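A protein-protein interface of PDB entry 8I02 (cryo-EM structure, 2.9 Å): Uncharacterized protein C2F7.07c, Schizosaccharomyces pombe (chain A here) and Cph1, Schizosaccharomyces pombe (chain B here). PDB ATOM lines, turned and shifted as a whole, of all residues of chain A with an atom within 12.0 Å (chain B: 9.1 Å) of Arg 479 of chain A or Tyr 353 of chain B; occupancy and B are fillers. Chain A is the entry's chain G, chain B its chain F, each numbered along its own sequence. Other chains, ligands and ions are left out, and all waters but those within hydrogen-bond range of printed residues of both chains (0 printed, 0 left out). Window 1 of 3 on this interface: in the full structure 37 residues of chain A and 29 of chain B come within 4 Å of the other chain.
The side-chain carboxylate (OD1) of Asp 350 of chain B lies within salt-bridge range of the guanidinium group (NE) of Arg 479 of chain A, at 3.4 Å.
The side-chain carboxylate (OD2) of Asp 350 of chain B lies within hydrogen-bond range of the backbone NH (N) of Gly 480 of chain A (3.5 Å).
O of Gly 476 of chain A sits close to O of Ser 176 of chain B.
Arg 474 of chain A touches Leu 175 of chain B.
Val 475 of chain A touches Leu 175 of chain B (O to CD2, 3.1 Å).
CA of Gly 476 of chain A touches CG of Leu 175 of chain B, at 3.7 Å.
Ile 177 of chain B touches Gly 476 of chain A (CA to O, 3.5 Å).
Ile 177 of chain B touches Pro 478 of chain A (CG1 to CD, 3.8 Å).
NH2 of Arg 479 of chain A touches O of Lys 349 of chain B, at 3.8 Å.
NH2 of Arg 479 of chain A touches CB of Tyr 353 of chain B, 3.6 Å away.
Val 342 of chain B touches Ile 487 of chain A (CG1 to CG2, 3.7 Å).
Of the printed residues of chain B, Val 475 of chain A touches Leu 175 (3.1 Å).
Of the printed residues of chain B, Pro 478 of chain A touches Ile 177.
Of chain B, only Lys 349 (3.8 Å), Asp 350 (3.1 Å) and Tyr 353 (3.6 Å) come within 4 Å of Arg 479 of chain A.
Printed residues of chain A within 4 Å of Leu 175 of chain B: Arg 474, Val 475 and Gly 476.
Printed residues of chain A within 4 Å of Ser 176 of chain B: Gly 476 (3.3 Å).
Printed residues of chain A within 4 Å of Ile 177 of chain B: Gly 476 and Pro 478.
No residue of chain A comes within 4 Å of Gly 346 of chain B.
Ile 348 of chain B touches none of the printed residues of chain A.
Lys 349 of chain B touches one residue of chain A.
No residue of chain A comes within 4 Å of Phe 351 of chain B.
No residue of chain A comes within 4 Å of Leu 352 of chain B.
No residue of chain A comes within 4 Å of Ile 355 of chain B.
No residue of chain A comes within 4 Å of Gly 356 of chain B.
No residue of chain A comes within 4 Å of Ile 357 of chain B.
Glu 358 of chain B touches none of the printed residues of chain A.
The nearest printed residue of chain B that does not touch Ile 487 of chain A is Leu 347 of chain B (4.6 Å).
Hydrophobic or aromatic side chains of chain A that line the printed part of chain B: Pro 478 and Ile 487.
Of the 21 printed residues of chain B, 7 touch a printed residue of chain A.
Among the printed residues, 11 pairs touch across the chains.
Among the printed residues, Asp or Glu carboxylates within 4 Å of a Lys or Arg side-chain nitrogen of the other chain: Arg 479 of chain A with Asp 350 of chain B.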
ATOM      1  N   ARG A 474      16.203  -1.357 -28.363  1.00  0.00           N
ATOM      2  CA  ARG A 474      17.472  -1.659 -27.702  1.00  0.00           C
ATOM      3  C   ARG A 474      17.509  -0.956 -26.355  1.00  0.00           C
ATOM      4  O   ARG A 474      17.721   0.251 -26.277  1.00  0.00           O
ATOM      5  CB  ARG A 474      18.646  -1.230 -28.566  1.00  0.00           C
ATOM      6  CG  ARG A 474      18.636  -1.809 -29.959  1.00  0.00           C
ATOM      7  CD  ARG A 474      19.938  -1.526 -30.691  1.00  0.00           C
ATOM      8  NE  ARG A 474      21.106  -2.046 -29.983  1.00  0.00           N
ATOM      9  CZ  ARG A 474      22.086  -1.291 -29.500  1.00  0.00           C
ATOM     10  NH1 ARG A 474      22.054   0.023 -29.654  1.00  0.00           N
ATOM     11  NH2 ARG A 474      23.109  -1.853 -28.875  1.00  0.00           N
ATOM     12  N   VAL A 475      17.319  -1.720 -25.284  1.00  0.00           N
ATOM     13  CA  VAL A 475      17.233  -1.173 -23.934  1.00  0.00           C
ATOM     14  C   VAL A 475      18.644  -0.819 -23.476  1.00  0.00           C
ATOM     15  O   VAL A 475      19.398  -1.694 -23.050  1.00  0.00           O
ATOM     16  CB  VAL A 475      16.572  -2.156 -22.970  1.00  0.00           C
ATOM     17  CG1 VAL A 475      16.700  -1.664 -21.541  1.00  0.00           C
ATOM     18  CG2 VAL A 475      15.137  -2.370 -23.346  1.00  0.00           C
ATOM     19  N   GLY A 476      19.002   0.461 -23.539  1.00  0.00           N
ATOM     20  CA  GLY A 476      20.203   0.900 -22.856  1.00  0.00           C
ATOM     21  C   GLY A 476      19.870   1.403 -21.469  1.00  0.00           C
ATOM     22  O   GLY A 476      19.537   2.572 -21.293  1.00  0.00           O
ATOM     23  N   LEU A 477      19.937   0.529 -20.485  1.00  0.00           N
ATOM     24  CA  LEU A 477      19.598   0.865 -19.112  1.00  0.00           C
ATOM     25  C   LEU A 477      20.256  -0.173 -18.216  1.00  0.00           C
ATOM     26  O   LEU A 477      19.684  -1.245 -17.984  1.00  0.00           O
ATOM     27  CB  LEU A 477      18.086   0.895 -18.914  1.00  0.00           C
ATOM     28  CG  LEU A 477      17.606   1.073 -17.479  1.00  0.00           C
ATOM     29  CD1 LEU A 477      18.045   2.404 -16.957  1.00  0.00           C
ATOM     30  CD2 LEU A 477      16.111   0.941 -17.402  1.00  0.00           C
ATOM     31  N   PRO A 478      21.443   0.082 -17.710  1.00  0.00           N
ATOM     32  CA  PRO A 478      22.270  -1.041 -17.271  1.00  0.00           C
ATOM     33  C   PRO A 478      21.974  -1.553 -15.873  1.00  0.00           C
ATOM     34  O   PRO A 478      22.918  -1.905 -15.164  1.00  0.00           O
ATOM     35  CB  PRO A 478      23.682  -0.456 -17.354  1.00  0.00           C
ATOM     36  CG  PRO A 478      23.487   0.986 -17.040  1.00  0.00           C
ATOM     37  CD  PRO A 478      22.127   1.375 -17.541  1.00  0.00           C
ATOM     38  N   ARG A 479      20.704  -1.603 -15.472  1.00  0.00           N
ATOM     39  CA  ARG A 479      20.196  -2.454 -14.395  1.00  0.00           C
ATOM     40  C   ARG A 479      18.720  -2.116 -14.183  1.00  0.00           C
ATOM     41  O   ARG A 479      18.212  -1.123 -14.709  1.00  0.00           O
ATOM     42  CB  ARG A 479      20.987  -2.336 -13.084  1.00  0.00           C
ATOM     43  CG  ARG A 479      21.949  -3.525 -12.883  1.00  0.00           C
ATOM     44  CD  ARG A 479      22.885  -3.388 -11.705  1.00  0.00           C
ATOM     45  NE  ARG A 479      22.491  -4.260 -10.608  1.00  0.00           N
ATOM     46  CZ  ARG A 479      23.304  -4.665  -9.643  1.00  0.00           C
ATOM     47  NH1 ARG A 479      24.570  -4.286  -9.634  1.00  0.00           N
ATOM     48  NH2 ARG A 479      22.852  -5.452  -8.681  1.00  0.00           N
ATOM     49  N   GLY A 480      18.038  -2.967 -13.425  1.00  0.00           N
ATOM     50  CA  GLY A 480      16.692  -2.677 -12.939  1.00  0.00           C
ATOM     51  C   GLY A 480      15.610  -2.456 -13.978  1.00  0.00           C
ATOM     52  O   GLY A 480      14.688  -1.667 -13.744  1.00  0.00           O
ATOM     53  N   PHE A 481      15.675  -3.157 -15.104  1.00  0.00           N
ATOM     54  CA  PHE A 481      14.688  -3.017 -16.165  1.00  0.00           C
ATOM     55  C   PHE A 481      13.541  -3.996 -15.937  1.00  0.00           C
ATOM     56  O   PHE A 481      13.766  -5.208 -15.880  1.00  0.00           O
ATOM     57  CB  PHE A 481      15.353  -3.264 -17.515  1.00  0.00           C
ATOM     58  CG  PHE A 481      14.419  -3.189 -18.675  1.00  0.00           C
ATOM     59  CD1 PHE A 481      13.988  -1.972 -19.156  1.00  0.00           C
ATOM     60  CD2 PHE A 481      13.984  -4.333 -19.299  1.00  0.00           C
ATOM     61  CE1 PHE A 481      13.130  -1.907 -20.226  1.00  0.00           C
ATOM     62  CE2 PHE A 481      13.132  -4.266 -20.365  1.00  0.00           C
ATOM     63  CZ  PHE A 481      12.704  -3.053 -20.825  1.00  0.00           C
ATOM     64  N   LYS A 482      12.315  -3.476 -15.804  1.00  0.00           N
ATOM     65  CA  LYS A 482      11.133  -4.299 -15.565  1.00  0.00           C
ATOM     66  C   LYS A 482      10.510  -4.741 -16.877  1.00  0.00           C
ATOM     67  O   LYS A 482      10.415  -3.955 -17.819  1.00  0.00           O
ATOM     68  CB  LYS A 482      10.073  -3.542 -14.765  1.00  0.00           C
ATOM     69  CG  LYS A 482      10.538  -2.924 -13.477  1.00  0.00           C
ATOM     70  CD  LYS A 482      11.184  -3.941 -12.575  1.00  0.00           C
ATOM     71  CE  LYS A 482      11.018  -3.550 -11.120  1.00  0.00           C
ATOM     72  NZ  LYS A 482      11.245  -2.099 -10.903  1.00  0.00           N
ATOM     73  N   ASN A 483      10.051  -5.985 -16.923  1.00  0.00           N
ATOM     74  CA  ASN A 483       9.296  -6.483 -18.068  1.00  0.00           C
ATOM     75  C   ASN A 483       8.548  -7.732 -17.628  1.00  0.00           C
ATOM     76  O   ASN A 483       8.475  -8.040 -16.435  1.00  0.00           O
ATOM     77  CB  ASN A 483      10.209  -6.729 -19.276  1.00  0.00           C
ATOM     78  CG  ASN A 483      11.211  -7.838 -19.046  1.00  0.00           C
ATOM     79  OD1 ASN A 483      11.714  -8.034 -17.945  1.00  0.00           O
ATOM     80  ND2 ASN A 483      11.524  -8.554 -20.101  1.00  0.00           N
ATOM     81  N   ILE A 487      11.821 -10.262 -24.122  1.00  0.00           N
ATOM     82  CA  ILE A 487      13.180  -9.783 -24.343  1.00  0.00           C
ATOM     83  C   ILE A 487      13.919 -10.703 -25.299  1.00  0.00           C
ATOM     84  O   ILE A 487      13.907 -11.925 -25.132  1.00  0.00           O
ATOM     85  CB  ILE A 487      13.957  -9.671 -23.024  1.00  0.00           C
ATOM     86  CG1 ILE A 487      13.667 -10.875 -22.133  1.00  0.00           C
ATOM     87  CG2 ILE A 487      13.617  -8.382 -22.342  1.00  0.00           C
ATOM     88  CD1 ILE A 487      14.752 -11.198 -21.144  1.00  0.00           C
ATOM     89  N   LEU B 175      26.307  -0.207 -24.845  1.00  0.00           N
ATOM     90  CA  LEU B 175      24.972  -0.013 -24.293  1.00  0.00           C
ATOM     91  C   LEU B 175      25.076   0.660 -22.926  1.00  0.00           C
ATOM     92  O   LEU B 175      25.487   0.034 -21.943  1.00  0.00           O
ATOM     93  CB  LEU B 175      24.230  -1.344 -24.203  1.00  0.00           C
ATOM     94  CG  LEU B 175      22.724  -1.291 -24.474  1.00  0.00           C
ATOM     95  CD1 LEU B 175      22.454  -0.718 -25.856  1.00  0.00           C
ATOM     96  CD2 LEU B 175      22.094  -2.658 -24.335  1.00  0.00           C
ATOM     97  N   SER B 176      24.709   1.937 -22.872  1.00  0.00           N
ATOM     98  CA  SER B 176      24.478   2.662 -21.633  1.00  0.00           C
ATOM     99  C   SER B 176      23.237   3.516 -21.850  1.00  0.00           C
ATOM    100  O   SER B 176      22.499   3.319 -22.817  1.00  0.00           O
ATOM    101  CB  SER B 176      25.707   3.485 -21.235  1.00  0.00           C
ATOM    102  OG  SER B 176      25.555   4.843 -21.594  1.00  0.00           O
ATOM    103  N   ILE B 177      22.989   4.475 -20.962  1.00  0.00           N
ATOM    104  CA  ILE B 177      21.744   5.225 -21.078  1.00  0.00           C
ATOM    105  C   ILE B 177      21.780   6.194 -22.255  1.00  0.00           C
ATOM    106  O   ILE B 177      20.741   6.492 -22.853  1.00  0.00           O
ATOM    107  CB  ILE B 177      21.438   5.952 -19.762  1.00  0.00           C
ATOM    108  CG1 ILE B 177      21.744   5.045 -18.581  1.00  0.00           C
ATOM    109  CG2 ILE B 177      19.989   6.351 -19.715  1.00  0.00           C
ATOM    110  CD1 ILE B 177      21.309   5.612 -17.271  1.00  0.00           C
ATOM    111  N   VAL B 342      18.325  -6.854 -24.405  1.00  0.00           N
ATOM    112  CA  VAL B 342      18.968  -6.689 -23.117  1.00  0.00           C
ATOM    113  C   VAL B 342      20.439  -7.041 -23.275  1.00  0.00           C
ATOM    114  O   VAL B 342      20.872  -7.550 -24.306  1.00  0.00           O
ATOM    115  CB  VAL B 342      18.312  -7.555 -22.027  1.00  0.00           C
ATOM    116  CG1 VAL B 342      16.969  -6.980 -21.618  1.00  0.00           C
ATOM    117  CG2 VAL B 342      18.146  -8.955 -22.530  1.00  0.00           C
ATOM    118  N   SER B 343      21.209  -6.749 -22.236  1.00  0.00           N
ATOM    119  CA  SER B 343      22.609  -7.128 -22.166  1.00  0.00           C
ATOM    120  C   SER B 343      22.758  -8.274 -21.184  1.00  0.00           C
ATOM    121  O   SER B 343      22.066  -8.319 -20.164  1.00  0.00           O
ATOM    122  CB  SER B 343      23.486  -5.955 -21.733  1.00  0.00           C
ATOM    123  OG  SER B 343      23.481  -4.930 -22.705  1.00  0.00           O
ATOM    124  N   ASP B 345      25.231  -9.030 -19.163  1.00  0.00           N
ATOM    125  CA  ASP B 345      25.913  -8.774 -17.897  1.00  0.00           C
ATOM    126  C   ASP B 345      25.028  -8.047 -16.893  1.00  0.00           C
ATOM    127  O   ASP B 345      25.072  -8.351 -15.696  1.00  0.00           O
ATOM    128  CB  ASP B 345      27.199  -7.995 -18.155  1.00  0.00           C
ATOM    129  CG  ASP B 345      27.079  -7.056 -19.326  1.00  0.00           C
ATOM    130  OD1 ASP B 345      26.718  -7.521 -20.423  1.00  0.00           O
ATOM    131  OD2 ASP B 345      27.347  -5.853 -19.153  1.00  0.00           O
ATOM    132  N   GLY B 346      24.228  -7.082 -17.348  1.00  0.00           N
ATOM    133  CA  GLY B 346      23.252  -6.477 -16.457  1.00  0.00           C
ATOM    134  C   GLY B 346      22.242  -7.492 -15.965  1.00  0.00           C
ATOM    135  O   GLY B 346      21.855  -7.484 -14.793  1.00  0.00           O
ATOM    136  N   LEU B 347      21.838  -8.406 -16.847  1.00  0.00           N
ATOM    137  CA  LEU B 347      20.963  -9.507 -16.464  1.00  0.00           C
ATOM    138  C   LEU B 347      21.615 -10.391 -15.410  1.00  0.00           C
ATOM    139  O   LEU B 347      20.966 -10.797 -14.441  1.00  0.00           O
ATOM    140  CB  LEU B 347      20.619 -10.314 -17.712  1.00  0.00           C
ATOM    141  CG  LEU B 347      19.277 -11.013 -17.877  1.00  0.00           C
ATOM    142  CD1 LEU B 347      19.029 -11.248 -19.350  1.00  0.00           C
ATOM    143  CD2 LEU B 347      19.283 -12.313 -17.129  1.00  0.00           C
ATOM    144  N   ILE B 348      22.902 -10.692 -15.578  1.00  0.00           N
ATOM    145  CA  ILE B 348      23.597 -11.582 -14.653  1.00  0.00           C
ATOM    146  C   ILE B 348      23.752 -10.931 -13.284  1.00  0.00           C
ATOM    147  O   ILE B 348      23.602 -11.588 -12.247  1.00  0.00           O
ATOM    148  CB  ILE B 348      24.953 -11.982 -15.250  1.00  0.00           C
ATOM    149  CG1 ILE B 348      24.748 -12.955 -16.405  1.00  0.00           C
ATOM    150  CG2 ILE B 348      25.848 -12.578 -14.183  1.00  0.00           C
ATOM    151  CD1 ILE B 348      25.884 -12.987 -17.382  1.00  0.00           C
ATOM    152  N   LYS B 349      24.063  -9.634 -13.253  1.00  0.00           N
ATOM    153  CA  LYS B 349      24.199  -8.947 -11.973  1.00  0.00           C
ATOM    154  C   LYS B 349      22.852  -8.806 -11.284  1.00  0.00           C
ATOM    155  O   LYS B 349      22.756  -8.951 -10.055  1.00  0.00           O
ATOM    156  CB  LYS B 349      24.862  -7.591 -12.174  1.00  0.00           C
ATOM    157  CG  LYS B 349      26.362  -7.692 -12.335  1.00  0.00           C
ATOM    158  CD  LYS B 349      26.986  -6.377 -12.749  1.00  0.00           C
ATOM    159  CE  LYS B 349      26.608  -5.999 -14.162  1.00  0.00           C
ATOM    160  NZ  LYS B 349      27.502  -4.942 -14.698  1.00  0.00           N
ATOM    161  N   ASP B 350      21.793  -8.562 -12.063  1.00  0.00           N
ATOM    162  CA  ASP B 350      20.439  -8.582 -11.519  1.00  0.00           C
ATOM    163  C   ASP B 350      20.118  -9.923 -10.882  1.00  0.00           C
ATOM    164  O   ASP B 350      19.580  -9.980  -9.769  1.00  0.00           O
ATOM    165  CB  ASP B 350      19.432  -8.271 -12.619  1.00  0.00           C
ATOM    166  CG  ASP B 350      19.361  -6.804 -12.936  1.00  0.00           C
ATOM    167  OD1 ASP B 350      20.144  -6.038 -12.347  1.00  0.00           O
ATOM    168  OD2 ASP B 350      18.520  -6.415 -13.767  1.00  0.00           O
ATOM    169  N   PHE B 351      20.441 -11.018 -11.573  1.00  0.00           N
ATOM    170  CA  PHE B 351      20.124 -12.332 -11.028  1.00  0.00           C
ATOM    171  C   PHE B 351      20.906 -12.605  -9.754  1.00  0.00           C
ATOM    172  O   PHE B 351      20.351 -13.118  -8.775  1.00  0.00           O
ATOM    173  CB  PHE B 351      20.391 -13.435 -12.051  1.00  0.00           C
ATOM    174  CG  PHE B 351      20.160 -14.815 -11.497  1.00  0.00           C
ATOM    175  CD1 PHE B 351      18.886 -15.228 -11.158  1.00  0.00           C
ATOM    176  CD2 PHE B 351      21.214 -15.678 -11.267  1.00  0.00           C
ATOM    177  CE1 PHE B 351      18.669 -16.469 -10.634  1.00  0.00           C
ATOM    178  CE2 PHE B 351      20.992 -16.922 -10.735  1.00  0.00           C
ATOM    179  CZ  PHE B 351      19.719 -17.312 -10.420  1.00  0.00           C
ATOM    180  N   LEU B 352      22.202 -12.284  -9.749  1.00  0.00           N
ATOM    181  CA  LEU B 352      23.010 -12.547  -8.565  1.00  0.00           C
ATOM    182  C   LEU B 352      22.509 -11.752  -7.368  1.00  0.00           C
ATOM    183  O   LEU B 352      22.450 -12.269  -6.249  1.00  0.00           O
ATOM    184  CB  LEU B 352      24.475 -12.230  -8.848  1.00  0.00           C
ATOM    185  CG  LEU B 352      25.232 -13.166  -9.787  1.00  0.00           C
ATOM    186  CD1 LEU B 352      26.639 -12.661  -9.954  1.00  0.00           C
ATOM    187  CD2 LEU B 352      25.239 -14.580  -9.255  1.00  0.00           C
ATOM    188  N   TYR B 353      22.113 -10.499  -7.596  1.00  0.00           N
ATOM    189  CA  TYR B 353      21.547  -9.690  -6.522  1.00  0.00           C
ATOM    190  C   TYR B 353      20.265 -10.311  -5.981  1.00  0.00           C
ATOM    191  O   TYR B 353      20.117 -10.507  -4.765  1.00  0.00           O
ATOM    192  CB  TYR B 353      21.297  -8.272  -7.039  1.00  0.00           C
ATOM    193  CG  TYR B 353      20.765  -7.327  -5.998  1.00  0.00           C
ATOM    194  CD1 TYR B 353      21.252  -7.349  -4.704  1.00  0.00           C
ATOM    195  CD2 TYR B 353      19.785  -6.406  -6.308  1.00  0.00           C
ATOM    196  CE1 TYR B 353      20.768  -6.497  -3.747  1.00  0.00           C
ATOM    197  CE2 TYR B 353      19.297  -5.544  -5.357  1.00  0.00           C
ATOM    198  CZ  TYR B 353      19.795  -5.592  -4.078  1.00  0.00           C
ATOM    199  OH  TYR B 353      19.314  -4.732  -3.120  1.00  0.00           O
ATOM    200  N   ALA B 354      19.328 -10.635  -6.875  1.00  0.00           N
ATOM    201  CA  ALA B 354      18.042 -11.169  -6.440  1.00  0.00           C
ATOM    202  C   ALA B 354      18.206 -12.466  -5.662  1.00  0.00           C
ATOM    203  O   ALA B 354      17.580 -12.663  -4.610  1.00  0.00           O
ATOM    204  CB  ALA B 354      17.140 -11.380  -7.652  1.00  0.00           C
ATOM    205  N   ILE B 355      19.065 -13.358  -6.150  1.00  0.00           N
ATOM    206  CA  ILE B 355      19.186 -14.650  -5.497  1.00  0.00           C
ATOM    207  C   ILE B 355      19.988 -14.543  -4.209  1.00  0.00           C
ATOM    208  O   ILE B 355      19.744 -15.304  -3.272  1.00  0.00           O
ATOM    209  CB  ILE B 355      19.769 -15.695  -6.463  1.00  0.00           C
ATOM    210  CG1 ILE B 355      19.457 -17.097  -5.953  1.00  0.00           C
ATOM    211  CG2 ILE B 355      21.244 -15.504  -6.661  1.00  0.00           C
ATOM    212  CD1 ILE B 355      17.989 -17.350  -5.717  1.00  0.00           C
ATOM    213  N   GLY B 356      20.924 -13.598  -4.108  1.00  0.00           N
ATOM    214  CA  GLY B 356      21.554 -13.356  -2.823  1.00  0.00           C
ATOM    215  C   GLY B 356      20.561 -12.896  -1.779  1.00  0.00           C
ATOM    216  O   GLY B 356      20.595 -13.350  -0.631  1.00  0.00           O
ATOM    217  N   ILE B 357      19.653 -12.001  -2.167  1.00  0.00           N
ATOM    218  CA  ILE B 357      18.613 -11.551  -1.240  1.00  0.00           C
ATOM    219  C   ILE B 357      17.760 -12.728  -0.779  1.00  0.00           C
ATOM    220  O   ILE B 357      17.536 -12.927   0.424  1.00  0.00           O
ATOM    221  CB  ILE B 357      17.747 -10.461  -1.892  1.00  0.00           C
ATOM    222  CG1 ILE B 357      18.603  -9.278  -2.335  1.00  0.00           C
ATOM    223  CG2 ILE B 357      16.672 -10.005  -0.927  1.00  0.00           C
ATOM    224  CD1 ILE B 357      17.804  -8.189  -2.971  1.00  0.00           C
ATOM    225  N   GLU B 358      17.273 -13.531  -1.731  1.00  0.00           N
ATOM    226  CA  GLU B 358      16.421 -14.664  -1.371  1.00  0.00           C
ATOM    227  C   GLU B 358      17.152 -15.668  -0.485  1.00  0.00           C
ATOM    228  O   GLU B 358      16.562 -16.214   0.455  1.00  0.00           O
ATOM    229  CB  GLU B 358      15.905 -15.359  -2.626  1.00  0.00           C
ATOM    230  CG  GLU B 358      14.687 -14.721  -3.246  1.00  0.00           C
ATOM    231  CD  GLU B 358      13.723 -15.746  -3.817  1.00  0.00           C
ATOM    232  OE1 GLU B 358      13.368 -16.703  -3.104  1.00  0.00           O
ATOM    233  OE2 GLU B 358      13.334 -15.603  -4.991  1.00  0.00           O
ATOM    234  N   ALA B 359      18.424 -15.946  -0.777  1.00  0.00           N
ATOM    235  CA  ALA B 359      19.153 -16.930   0.011  1.00  0.00           C
ATOM    236  C   ALA B 359      19.399 -16.428   1.427  1.00  0.00           C
ATOM    237  O   ALA B 359      19.277 -17.193   2.394  1.00  0.00           O
ATOM    238  CB  ALA B 359      20.463 -17.281  -0.683  1.00  0.00           C
ATOM    239  N   LYS B 360      19.744 -15.147   1.572  1.00  0.00           N
ATOM    240  CA  LYS B 360      19.840 -14.562   2.904  1.00  0.00           C
ATOM    241  C   LYS B 360      18.523 -14.692   3.655  1.00  0.00           C
ATOM    242  O   LYS B 360      18.512 -14.930   4.867  1.00  0.00           O
ATOM    243  CB  LYS B 360      20.255 -13.097   2.802  1.00  0.00           C
ATOM    244  CG  LYS B 360      20.017 -12.287   4.057  1.00  0.00           C
ATOM    245  CD  LYS B 360      19.909 -10.807   3.743  1.00  0.00           C
ATOM    246  CE  LYS B 360      18.785 -10.524   2.755  1.00  0.00           C
ATOM    247  NZ  LYS B 360      17.457 -10.913   3.291  1.00  0.00           N
